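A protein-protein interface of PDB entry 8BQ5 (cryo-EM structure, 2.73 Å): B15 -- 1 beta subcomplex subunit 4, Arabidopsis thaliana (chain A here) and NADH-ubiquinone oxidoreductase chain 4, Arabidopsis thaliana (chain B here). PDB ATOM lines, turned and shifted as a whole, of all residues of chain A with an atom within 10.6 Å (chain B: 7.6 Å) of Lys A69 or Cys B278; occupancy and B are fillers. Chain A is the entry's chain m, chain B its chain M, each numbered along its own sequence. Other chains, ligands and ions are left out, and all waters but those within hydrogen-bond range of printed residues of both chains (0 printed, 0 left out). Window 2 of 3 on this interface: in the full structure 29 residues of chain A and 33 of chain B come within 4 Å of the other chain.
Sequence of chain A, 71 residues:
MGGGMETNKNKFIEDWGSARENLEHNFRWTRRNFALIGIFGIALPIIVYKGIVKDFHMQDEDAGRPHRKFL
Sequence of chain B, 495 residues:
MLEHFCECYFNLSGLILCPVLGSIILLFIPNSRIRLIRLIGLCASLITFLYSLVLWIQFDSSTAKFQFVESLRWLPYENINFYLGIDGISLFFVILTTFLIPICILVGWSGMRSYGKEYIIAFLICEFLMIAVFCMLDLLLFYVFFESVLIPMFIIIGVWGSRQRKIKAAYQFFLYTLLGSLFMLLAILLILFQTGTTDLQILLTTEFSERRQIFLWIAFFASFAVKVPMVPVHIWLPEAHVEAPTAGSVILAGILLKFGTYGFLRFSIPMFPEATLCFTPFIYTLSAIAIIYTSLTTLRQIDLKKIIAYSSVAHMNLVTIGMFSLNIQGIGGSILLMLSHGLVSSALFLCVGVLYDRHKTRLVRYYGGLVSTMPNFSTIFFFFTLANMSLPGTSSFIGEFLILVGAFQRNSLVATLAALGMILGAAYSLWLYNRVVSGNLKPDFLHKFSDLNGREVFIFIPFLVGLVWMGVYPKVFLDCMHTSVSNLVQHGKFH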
ATOM      1  N   TYR A  49     -14.897 -36.987  25.739  1.00  0.00           N
ATOM      2  CA  TYR A  49     -14.918 -35.919  24.745  1.00  0.00           C
ATOM      3  C   TYR A  49     -15.641 -36.359  23.477  1.00  0.00           C
ATOM      4  O   TYR A  49     -16.393 -35.585  22.875  1.00  0.00           O
ATOM      5  CB  TYR A  49     -13.492 -35.468  24.428  1.00  0.00           C
ATOM      6  CG  TYR A  49     -13.414 -34.473  23.295  1.00  0.00           C
ATOM      7  CD1 TYR A  49     -13.601 -33.118  23.524  1.00  0.00           C
ATOM      8  CD2 TYR A  49     -13.155 -34.887  21.996  1.00  0.00           C
ATOM      9  CE1 TYR A  49     -13.537 -32.205  22.493  1.00  0.00           C
ATOM     10  CE2 TYR A  49     -13.089 -33.981  20.959  1.00  0.00           C
ATOM     11  CZ  TYR A  49     -13.281 -32.642  21.214  1.00  0.00           C
ATOM     12  OH  TYR A  49     -13.215 -31.736  20.183  1.00  0.00           O
ATOM     13  N   ILE A  52     -19.353 -36.458  24.061  1.00  0.00           N
ATOM     14  CA  ILE A  52     -19.928 -35.117  24.068  1.00  0.00           C
ATOM     15  C   ILE A  52     -20.044 -34.577  22.647  1.00  0.00           C
ATOM     16  O   ILE A  52     -21.059 -33.976  22.276  1.00  0.00           O
ATOM     17  CB  ILE A  52     -19.095 -34.185  24.969  1.00  0.00           C
ATOM     18  CG1 ILE A  52     -19.196 -34.632  26.428  1.00  0.00           C
ATOM     19  CG2 ILE A  52     -19.555 -32.744  24.824  1.00  0.00           C
ATOM     20  CD1 ILE A  52     -18.198 -33.968  27.348  1.00  0.00           C
ATOM     21  N   VAL A  53     -19.006 -34.779  21.833  1.00  0.00           N
ATOM     22  CA  VAL A  53     -19.044 -34.318  20.448  1.00  0.00           C
ATOM     23  C   VAL A  53     -20.113 -35.068  19.661  1.00  0.00           C
ATOM     24  O   VAL A  53     -20.864 -34.469  18.881  1.00  0.00           O
ATOM     25  CB  VAL A  53     -17.655 -34.463  19.798  1.00  0.00           C
ATOM     26  CG1 VAL A  53     -17.757 -34.352  18.286  1.00  0.00           C
ATOM     27  CG2 VAL A  53     -16.709 -33.411  20.337  1.00  0.00           C
ATOM     28  N   LYS A  54     -20.200 -36.385  19.854  1.00  0.00           N
ATOM     29  CA  LYS A  54     -21.209 -37.172  19.151  1.00  0.00           C
ATOM     30  C   LYS A  54     -22.613 -36.737  19.552  1.00  0.00           C
ATOM     31  O   LYS A  54     -23.541 -36.771  18.736  1.00  0.00           O
ATOM     32  CB  LYS A  54     -20.992 -38.659  19.434  1.00  0.00           C
ATOM     33  CG  LYS A  54     -22.216 -39.536  19.247  1.00  0.00           C
ATOM     34  CD  LYS A  54     -22.311 -40.014  17.811  1.00  0.00           C
ATOM     35  CE  LYS A  54     -21.334 -41.148  17.552  1.00  0.00           C
ATOM     36  NZ  LYS A  54     -20.946 -41.239  16.119  1.00  0.00           N
ATOM     37  N   PHE A  56     -23.538 -33.673  20.177  1.00  0.00           N
ATOM     38  CA  PHE A  56     -23.823 -32.534  19.310  1.00  0.00           C
ATOM     39  C   PHE A  56     -24.132 -32.982  17.888  1.00  0.00           C
ATOM     40  O   PHE A  56     -25.086 -32.495  17.270  1.00  0.00           O
ATOM     41  CB  PHE A  56     -22.644 -31.560  19.301  1.00  0.00           C
ATOM     42  CG  PHE A  56     -22.519 -30.732  20.547  1.00  0.00           C
ATOM     43  CD1 PHE A  56     -23.567 -29.933  20.976  1.00  0.00           C
ATOM     44  CD2 PHE A  56     -21.342 -30.729  21.274  1.00  0.00           C
ATOM     45  CE1 PHE A  56     -23.446 -29.162  22.117  1.00  0.00           C
ATOM     46  CE2 PHE A  56     -21.216 -29.961  22.415  1.00  0.00           C
ATOM     47  CZ  PHE A  56     -22.269 -29.177  22.836  1.00  0.00           C
ATOM     48  N   HIS A  57     -23.331 -33.908  17.350  1.00  0.00           N
ATOM     49  CA  HIS A  57     -23.518 -34.339  15.968  1.00  0.00           C
ATOM     50  C   HIS A  57     -24.879 -34.993  15.773  1.00  0.00           C
ATOM     51  O   HIS A  57     -25.523 -34.800  14.736  1.00  0.00           O
ATOM     52  CB  HIS A  57     -22.408 -35.306  15.559  1.00  0.00           C
ATOM     53  CG  HIS A  57     -21.085 -34.649  15.326  1.00  0.00           C
ATOM     54  ND1 HIS A  57     -19.930 -35.366  15.098  1.00  0.00           N
ATOM     55  CD2 HIS A  57     -20.730 -33.344  15.300  1.00  0.00           C
ATOM     56  CE1 HIS A  57     -18.922 -34.529  14.932  1.00  0.00           C
ATOM     57  NE2 HIS A  57     -19.379 -33.296  15.052  1.00  0.00           N
ATOM     58  N   ASP A  60     -27.240 -32.466  15.394  1.00  0.00           N
ATOM     59  CA  ASP A  60     -27.118 -31.850  14.077  1.00  0.00           C
ATOM     60  C   ASP A  60     -27.955 -32.593  13.041  1.00  0.00           C
ATOM     61  O   ASP A  60     -28.745 -31.983  12.312  1.00  0.00           O
ATOM     62  CB  ASP A  60     -25.649 -31.805  13.658  1.00  0.00           C
ATOM     63  CG  ASP A  60     -25.005 -30.463  13.946  1.00  0.00           C
ATOM     64  OD1 ASP A  60     -25.747 -29.503  14.233  1.00  0.00           O
ATOM     65  OD2 ASP A  60     -23.761 -30.370  13.891  1.00  0.00           O
ATOM     66  N   ARG A  65     -29.038 -30.711   9.767  1.00  0.00           N
ATOM     67  CA  ARG A  65     -27.924 -29.797   9.577  1.00  0.00           C
ATOM     68  C   ARG A  65     -26.615 -30.569   9.552  1.00  0.00           C
ATOM     69  O   ARG A  65     -26.479 -31.590  10.233  1.00  0.00           O
ATOM     70  CB  ARG A  65     -27.880 -28.745  10.695  1.00  0.00           C
ATOM     71  CG  ARG A  65     -28.589 -27.445  10.353  1.00  0.00           C
ATOM     72  CD  ARG A  65     -28.412 -26.390  11.438  1.00  0.00           C
ATOM     73  NE  ARG A  65     -29.075 -26.763  12.684  1.00  0.00           N
ATOM     74  CZ  ARG A  65     -28.487 -27.388  13.695  1.00  0.00           C
ATOM     75  NH1 ARG A  65     -27.202 -27.699  13.663  1.00  0.00           N
ATOM     76  NH2 ARG A  65     -29.206 -27.704  14.768  1.00  0.00           N
ATOM     77  N   PRO A  66     -25.636 -30.104   8.780  1.00  0.00           N
ATOM     78  CA  PRO A  66     -24.350 -30.808   8.707  1.00  0.00           C
ATOM     79  C   PRO A  66     -23.630 -30.785  10.047  1.00  0.00           C
ATOM     80  O   PRO A  66     -23.852 -29.921  10.898  1.00  0.00           O
ATOM     81  CB  PRO A  66     -23.571 -30.034   7.638  1.00  0.00           C
ATOM     82  CG  PRO A  66     -24.602 -29.244   6.892  1.00  0.00           C
ATOM     83  CD  PRO A  66     -25.688 -28.947   7.872  1.00  0.00           C
ATOM     84  N   HIS A  67     -22.755 -31.773  10.225  1.00  0.00           N
ATOM     85  CA  HIS A  67     -22.050 -31.946  11.488  1.00  0.00           C
ATOM     86  C   HIS A  67     -21.228 -30.707  11.820  1.00  0.00           C
ATOM     87  O   HIS A  67     -20.600 -30.109  10.942  1.00  0.00           O
ATOM     88  CB  HIS A  67     -21.146 -33.176  11.424  1.00  0.00           C
ATOM     89  CG  HIS A  67     -21.842 -34.457  11.766  1.00  0.00           C
ATOM     90  ND1 HIS A  67     -21.159 -35.615  12.069  1.00  0.00           N
ATOM     91  CD2 HIS A  67     -23.157 -34.764  11.848  1.00  0.00           C
ATOM     92  CE1 HIS A  67     -22.024 -36.580  12.323  1.00  0.00           C
ATOM     93  NE2 HIS A  67     -23.244 -36.089  12.198  1.00  0.00           N
ATOM     94  N   ARG A  68     -21.237 -30.324  13.094  1.00  0.00           N
ATOM     95  CA  ARG A  68     -20.497 -29.147  13.526  1.00  0.00           C
ATOM     96  C   ARG A  68     -19.026 -29.485  13.712  1.00  0.00           C
ATOM     97  O   ARG A  68     -18.678 -30.437  14.417  1.00  0.00           O
ATOM     98  CB  ARG A  68     -21.081 -28.600  14.828  1.00  0.00           C
ATOM     99  CG  ARG A  68     -21.363 -27.107  14.800  1.00  0.00           C
ATOM    100  CD  ARG A  68     -22.113 -26.642  16.041  1.00  0.00           C
ATOM    101  NE  ARG A  68     -23.362 -27.368  16.237  1.00  0.00           N
ATOM    102  CZ  ARG A  68     -23.677 -28.037  17.338  1.00  0.00           C
ATOM    103  NH1 ARG A  68     -22.870 -28.060  18.386  1.00  0.00           N
ATOM    104  NH2 ARG A  68     -24.832 -28.693  17.391  1.00  0.00           N
ATOM    105  N   LYS A  69     -18.161 -28.712  13.066  1.00  0.00           N
ATOM    106  CA  LYS A  69     -16.733 -28.847  13.289  1.00  0.00           C
ATOM    107  C   LYS A  69     -16.381 -28.327  14.676  1.00  0.00           C
ATOM    108  O   LYS A  69     -17.000 -27.389  15.187  1.00  0.00           O
ATOM    109  CB  LYS A  69     -15.948 -28.091  12.216  1.00  0.00           C
ATOM    110  CG  LYS A  69     -16.067 -28.696  10.821  1.00  0.00           C
ATOM    111  CD  LYS A  69     -15.307 -27.868   9.795  1.00  0.00           C
ATOM    112  CE  LYS A  69     -15.434 -28.449   8.395  1.00  0.00           C
ATOM    113  NZ  LYS A  69     -14.717 -27.612   7.389  1.00  0.00           N
ATOM    114  N   PHE A  70     -15.381 -28.952  15.294  1.00  0.00           N
ATOM    115  CA  PHE A  70     -14.993 -28.614  16.654  1.00  0.00           C
ATOM    116  C   PHE A  70     -13.478 -28.641  16.781  1.00  0.00           C
ATOM    117  O   PHE A  70     -12.777 -29.195  15.930  1.00  0.00           O
ATOM    118  CB  PHE A  70     -15.636 -29.567  17.669  1.00  0.00           C
ATOM    119  CG  PHE A  70     -17.088 -29.285  17.921  1.00  0.00           C
ATOM    120  CD1 PHE A  70     -17.497 -28.026  18.323  1.00  0.00           C
ATOM    121  CD2 PHE A  70     -18.041 -30.270  17.744  1.00  0.00           C
ATOM    122  CE1 PHE A  70     -18.830 -27.758  18.555  1.00  0.00           C
ATOM    123  CE2 PHE A  70     -19.375 -30.008  17.972  1.00  0.00           C
ATOM    124  CZ  PHE A  70     -19.769 -28.751  18.379  1.00  0.00           C
ATOM    125  N   LEU A  71     -12.988 -28.026  17.856  1.00  0.00           N
ATOM    126  CA  LEU A  71     -11.560 -27.852  18.110  1.00  0.00           C
ATOM    127  C   LEU A  71     -10.903 -27.059  16.986  1.00  0.00           C
ATOM    128  O   LEU A  71     -11.315 -25.938  16.686  1.00  0.00           O
ATOM    129  CB  LEU A  71     -10.858 -29.203  18.286  1.00  0.00           C
ATOM    130  CG  LEU A  71     -10.676 -29.676  19.730  1.00  0.00           C
ATOM    131  CD1 LEU A  71      -9.703 -30.844  19.806  1.00  0.00           C
ATOM    132  CD2 LEU A  71     -10.225 -28.534  20.619  1.00  0.00           C
ATOM    133  N   GLU B 210     -11.349 -16.289  11.954  1.00  0.00           N
ATOM    134  CA  GLU B 210     -11.545 -17.561  12.642  1.00  0.00           C
ATOM    135  C   GLU B 210     -10.225 -18.112  13.171  1.00  0.00           C
ATOM    136  O   GLU B 210     -10.134 -18.516  14.334  1.00  0.00           O
ATOM    137  CB  GLU B 210     -12.232 -18.565  11.712  1.00  0.00           C
ATOM    138  CG  GLU B 210     -13.750 -18.410  11.668  1.00  0.00           C
ATOM    139  CD  GLU B 210     -14.448 -19.501  10.871  1.00  0.00           C
ATOM    140  OE1 GLU B 210     -13.757 -20.323  10.233  1.00  0.00           O
ATOM    141  OE2 GLU B 210     -15.698 -19.537  10.890  1.00  0.00           O
ATOM    142  N   ILE B 214      -9.293 -18.555  17.131  1.00  0.00           N
ATOM    143  CA  ILE B 214      -8.842 -19.779  17.789  1.00  0.00           C
ATOM    144  C   ILE B 214      -7.553 -19.528  18.566  1.00  0.00           C
ATOM    145  O   ILE B 214      -7.425 -19.925  19.733  1.00  0.00           O
ATOM    146  CB  ILE B 214      -8.682 -20.921  16.763  1.00  0.00           C
ATOM    147  CG1 ILE B 214     -10.012 -21.649  16.518  1.00  0.00           C
ATOM    148  CG2 ILE B 214      -7.619 -21.913  17.204  1.00  0.00           C
ATOM    149  CD1 ILE B 214     -11.119 -20.840  15.899  1.00  0.00           C
ATOM    150  N   TRP B 217      -8.125 -17.247  21.582  1.00  0.00           N
ATOM    151  CA  TRP B 217      -8.869 -18.026  22.604  1.00  0.00           C
ATOM    152  C   TRP B 217      -7.906 -18.906  23.402  1.00  0.00           C
ATOM    153  O   TRP B 217      -8.050 -18.923  24.617  1.00  0.00           O
ATOM    154  CB  TRP B 217      -9.964 -18.877  21.952  1.00  0.00           C
ATOM    155  CG  TRP B 217     -11.026 -19.355  22.893  1.00  0.00           C
ATOM    156  CD1 TRP B 217     -12.237 -18.774  23.127  1.00  0.00           C
ATOM    157  CD2 TRP B 217     -10.977 -20.527  23.726  1.00  0.00           C
ATOM    158  NE1 TRP B 217     -12.943 -19.499  24.047  1.00  0.00           N
ATOM    159  CE2 TRP B 217     -12.196 -20.579  24.432  1.00  0.00           C
ATOM    160  CE3 TRP B 217     -10.025 -21.528  23.950  1.00  0.00           C
ATOM    161  CZ2 TRP B 217     -12.480 -21.596  25.341  1.00  0.00           C
ATOM    162  CZ3 TRP B 217     -10.311 -22.538  24.839  1.00  0.00           C
ATOM    163  CH2 TRP B 217     -11.521 -22.562  25.528  1.00  0.00           C
ATOM    164  N   PHE B 272     -14.680 -13.620  21.115  1.00  0.00           N
ATOM    165  CA  PHE B 272     -14.425 -14.678  20.102  1.00  0.00           C
ATOM    166  C   PHE B 272     -15.602 -15.656  20.079  1.00  0.00           C
ATOM    167  O   PHE B 272     -15.445 -16.789  20.561  1.00  0.00           O
ATOM    168  CB  PHE B 272     -13.088 -15.380  20.365  1.00  0.00           C
ATOM    169  CG  PHE B 272     -11.996 -14.511  20.933  1.00  0.00           C
ATOM    170  CD1 PHE B 272     -11.471 -13.456  20.205  1.00  0.00           C
ATOM    171  CD2 PHE B 272     -11.483 -14.760  22.196  1.00  0.00           C
ATOM    172  CE1 PHE B 272     -10.475 -12.654  20.738  1.00  0.00           C
ATOM    173  CE2 PHE B 272     -10.481 -13.965  22.724  1.00  0.00           C
ATOM    174  CZ  PHE B 272      -9.978 -12.915  21.995  1.00  0.00           C
ATOM    175  N   PRO B 273     -16.772 -15.286  19.515  1.00  0.00           N
ATOM    176  CA  PRO B 273     -17.952 -16.163  19.564  1.00  0.00           C
ATOM    177  C   PRO B 273     -17.814 -17.433  18.742  1.00  0.00           C
ATOM    178  O   PRO B 273     -18.364 -18.470  19.132  1.00  0.00           O
ATOM    179  CB  PRO B 273     -19.074 -15.260  19.039  1.00  0.00           C
ATOM    180  CG  PRO B 273     -18.380 -14.273  18.176  1.00  0.00           C
ATOM    181  CD  PRO B 273     -17.043 -14.025  18.804  1.00  0.00           C
ATOM    182  N   GLU B 274     -17.106 -17.387  17.611  1.00  0.00           N
ATOM    183  CA  GLU B 274     -16.873 -18.612  16.850  1.00  0.00           C
ATOM    184  C   GLU B 274     -15.907 -19.536  17.579  1.00  0.00           C
ATOM    185  O   GLU B 274     -16.130 -20.750  17.643  1.00  0.00           O
ATOM    186  CB  GLU B 274     -16.347 -18.284  15.452  1.00  0.00           C
ATOM    187  CG  GLU B 274     -17.385 -17.723  14.490  1.00  0.00           C
ATOM    188  CD  GLU B 274     -17.873 -16.345  14.880  1.00  0.00           C
ATOM    189  OE1 GLU B 274     -19.019 -16.235  15.364  1.00  0.00           O
ATOM    190  OE2 GLU B 274     -17.112 -15.370  14.705  1.00  0.00           O
ATOM    191  N   ALA B 275     -14.833 -18.977  18.141  1.00  0.00           N
ATOM    192  CA  ALA B 275     -13.882 -19.791  18.891  1.00  0.00           C
ATOM    193  C   ALA B 275     -14.542 -20.426  20.106  1.00  0.00           C
ATOM    194  O   ALA B 275     -14.220 -21.560  20.477  1.00  0.00           O
ATOM    195  CB  ALA B 275     -12.681 -18.945  19.311  1.00  0.00           C
ATOM    196  N   THR B 276     -15.477 -19.711  20.736  1.00  0.00           N
ATOM    197  CA  THR B 276     -16.176 -20.258  21.893  1.00  0.00           C
ATOM    198  C   THR B 276     -16.940 -21.526  21.528  1.00  0.00           C
ATOM    199  O   THR B 276     -16.911 -22.513  22.272  1.00  0.00           O
ATOM    200  CB  THR B 276     -17.124 -19.208  22.476  1.00  0.00           C
ATOM    201  OG1 THR B 276     -16.362 -18.151  23.071  1.00  0.00           O
ATOM    202  CG2 THR B 276     -18.027 -19.823  23.529  1.00  0.00           C
ATOM    203  N   LEU B 277     -17.620 -21.521  20.379  1.00  0.00           N
ATOM    204  CA  LEU B 277     -18.418 -22.676  19.977  1.00  0.00           C
ATOM    205  C   LEU B 277     -17.534 -23.878  19.660  1.00  0.00           C
ATOM    206  O   LEU B 277     -17.838 -25.007  20.061  1.00  0.00           O
ATOM    207  CB  LEU B 277     -19.293 -22.309  18.775  1.00  0.00           C
ATOM    208  CG  LEU B 277     -20.188 -23.371  18.125  1.00  0.00           C
ATOM    209  CD1 LEU B 277     -20.730 -24.384  19.131  1.00  0.00           C
ATOM    210  CD2 LEU B 277     -21.337 -22.706  17.384  1.00  0.00           C
ATOM    211  N   CYS B 278     -16.432 -23.657  18.942  1.00  0.00           N
ATOM    212  CA  CYS B 278     -15.564 -24.768  18.563  1.00  0.00           C
ATOM    213  C   CYS B 278     -14.951 -25.439  19.786  1.00  0.00           C
ATOM    214  O   CYS B 278     -14.637 -26.634  19.756  1.00  0.00           O
ATOM    215  CB  CYS B 278     -14.471 -24.276  17.615  1.00  0.00           C
ATOM    216  SG  CYS B 278     -14.978 -24.178  15.882  1.00  0.00           S
ATOM    217  N   PHE B 279     -14.782 -24.692  20.873  1.00  0.00           N
ATOM    218  CA  PHE B 279     -14.126 -25.199  22.070  1.00  0.00           C
ATOM    219  C   PHE B 279     -15.097 -25.647  23.154  1.00  0.00           C
ATOM    220  O   PHE B 279     -14.647 -26.120  24.203  1.00  0.00           O
ATOM    221  CB  PHE B 279     -13.185 -24.135  22.639  1.00  0.00           C
ATOM    222  CG  PHE B 279     -11.895 -24.009  21.889  1.00  0.00           C
ATOM    223  CD1 PHE B 279     -11.016 -25.074  21.818  1.00  0.00           C
ATOM    224  CD2 PHE B 279     -11.563 -22.830  21.246  1.00  0.00           C
ATOM    225  CE1 PHE B 279      -9.829 -24.962  21.128  1.00  0.00           C
ATOM    226  CE2 PHE B 279     -10.376 -22.713  20.556  1.00  0.00           C
ATOM    227  CZ  PHE B 279      -9.508 -23.782  20.496  1.00  0.00           C
ATOM    228  N   THR B 280     -16.405 -25.512  22.936  1.00  0.00           N
ATOM    229  CA  THR B 280     -17.369 -25.915  23.960  1.00  0.00           C
ATOM    230  C   THR B 280     -17.256 -27.388  24.338  1.00  0.00           C
ATOM    231  O   THR B 280     -17.251 -27.687  25.545  1.00  0.00           O
ATOM    232  CB  THR B 280     -18.790 -25.558  23.509  1.00  0.00           C
ATOM    233  OG1 THR B 280     -18.879 -24.149  23.274  1.00  0.00           O
ATOM    234  CG2 THR B 280     -19.799 -25.954  24.571  1.00  0.00           C
ATOM    235  N   PRO B 281     -17.171 -28.346  23.403  1.00  0.00           N
ATOM    236  CA  PRO B 281     -16.949 -29.736  23.834  1.00  0.00           C
ATOM    237  C   PRO B 281     -15.669 -29.920  24.628  1.00  0.00           C
ATOM    238  O   PRO B 281     -15.639 -30.720  25.571  1.00  0.00           O
ATOM    239  CB  PRO B 281     -16.913 -30.509  22.509  1.00  0.00           C
ATOM    240  CG  PRO B 281     -17.680 -29.668  21.567  1.00  0.00           C
ATOM    241  CD  PRO B 281     -17.338 -28.264  21.941  1.00  0.00           C
ATOM    242  N   PHE B 282     -14.605 -29.200  24.268  1.00  0.00           N
ATOM    243  CA  PHE B 282     -13.352 -29.292  25.012  1.00  0.00           C
ATOM    244  C   PHE B 282     -13.517 -28.764  26.432  1.00  0.00           C
ATOM    245  O   PHE B 282     -13.018 -29.362  27.392  1.00  0.00           O
ATOM    246  CB  PHE B 282     -12.250 -28.531  24.277  1.00  0.00           C
ATOM    247  CG  PHE B 282     -10.956 -28.455  25.035  1.00  0.00           C
ATOM    248  CD1 PHE B 282     -10.181 -29.586  25.225  1.00  0.00           C
ATOM    249  CD2 PHE B 282     -10.519 -27.254  25.565  1.00  0.00           C
ATOM    250  CE1 PHE B 282      -8.994 -29.520  25.923  1.00  0.00           C
ATOM    251  CE2 PHE B 282      -9.332 -27.181  26.266  1.00  0.00           C
ATOM    252  CZ  PHE B 282      -8.568 -28.315  26.444  1.00  0.00           C
ATOM    253  N   ILE B 283     -14.212 -27.635  26.583  1.00  0.00           N
ATOM    254  CA  ILE B 283     -14.484 -27.095  27.913  1.00  0.00           C
ATOM    255  C   ILE B 283     -15.348 -28.063  28.707  1.00  0.00           C
ATOM    256  O   ILE B 283     -15.127 -28.281  29.905  1.00  0.00           O
ATOM    257  CB  ILE B 283     -15.141 -25.707  27.802  1.00  0.00           C
ATOM    258  CG1 ILE B 283     -14.133 -24.685  27.281  1.00  0.00           C
ATOM    259  CG2 ILE B 283     -15.692 -25.259  29.148  1.00  0.00           C
ATOM    260  CD1 ILE B 283     -12.950 -24.497  28.193  1.00  0.00           C
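The backbone carbonyl oxygen of Cys B278 sits at hydrogen-bond distance from the backbone NH of Leu A71, 2.9 Å away.
The backbone carbonyl oxygen (O) of Leu B277 sits at hydrogen-bond distance from the side-chain hydroxyl (OG1) of Thr B280 (3.5 Å).
Among the printed residues, merely in contact across the chains: Tyr A49 with Pro B281, Tyr A49 with Phe B282, Val A53 with Pro B281, Phe A56 with Pro B281, Lys A69 with Cys B278, Phe A70 with Leu B277, Phe A70 with Cys B278, Phe A70 with Pro B281 and Leu A71 with Phe B279.
Lys A69 touches just one residue of chain B: Cys B278.
Of chain A, only Lys A69, Phe A70 and Leu A71 come within 4 Å of Cys B278.
Phe B279 touches one residue of chain A.
Of the printed residues of chain B, Phe A56 touches Pro B281 (3.6 Å).
Printed residues of chain B within 4 Å of Phe A70: Leu B277, Cys B278 and Pro B281.
Of the printed residues of chain A, Pro B281 touches Tyr A49, Val A53, Phe A56 and Phe A70.
Printed residues of chain B within 4 Å of Val A53: Pro B281.
The nearest residue of chain B that does not touch Lys A69 is Leu B277 (5.5 Å).
The nearest printed residue of chain B that does not touch Phe A70 is Phe B279 (5.0 Å).
Hydrophobic or aromatic side chains of chain B within 4 Å of the printed part of chain A: Leu B277, Phe B279 and Pro B281.
Among the printed residues, no Asp or Glu carboxylate lies within 4 Å of a Lys or Arg side-chain nitrogen of the other chain.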
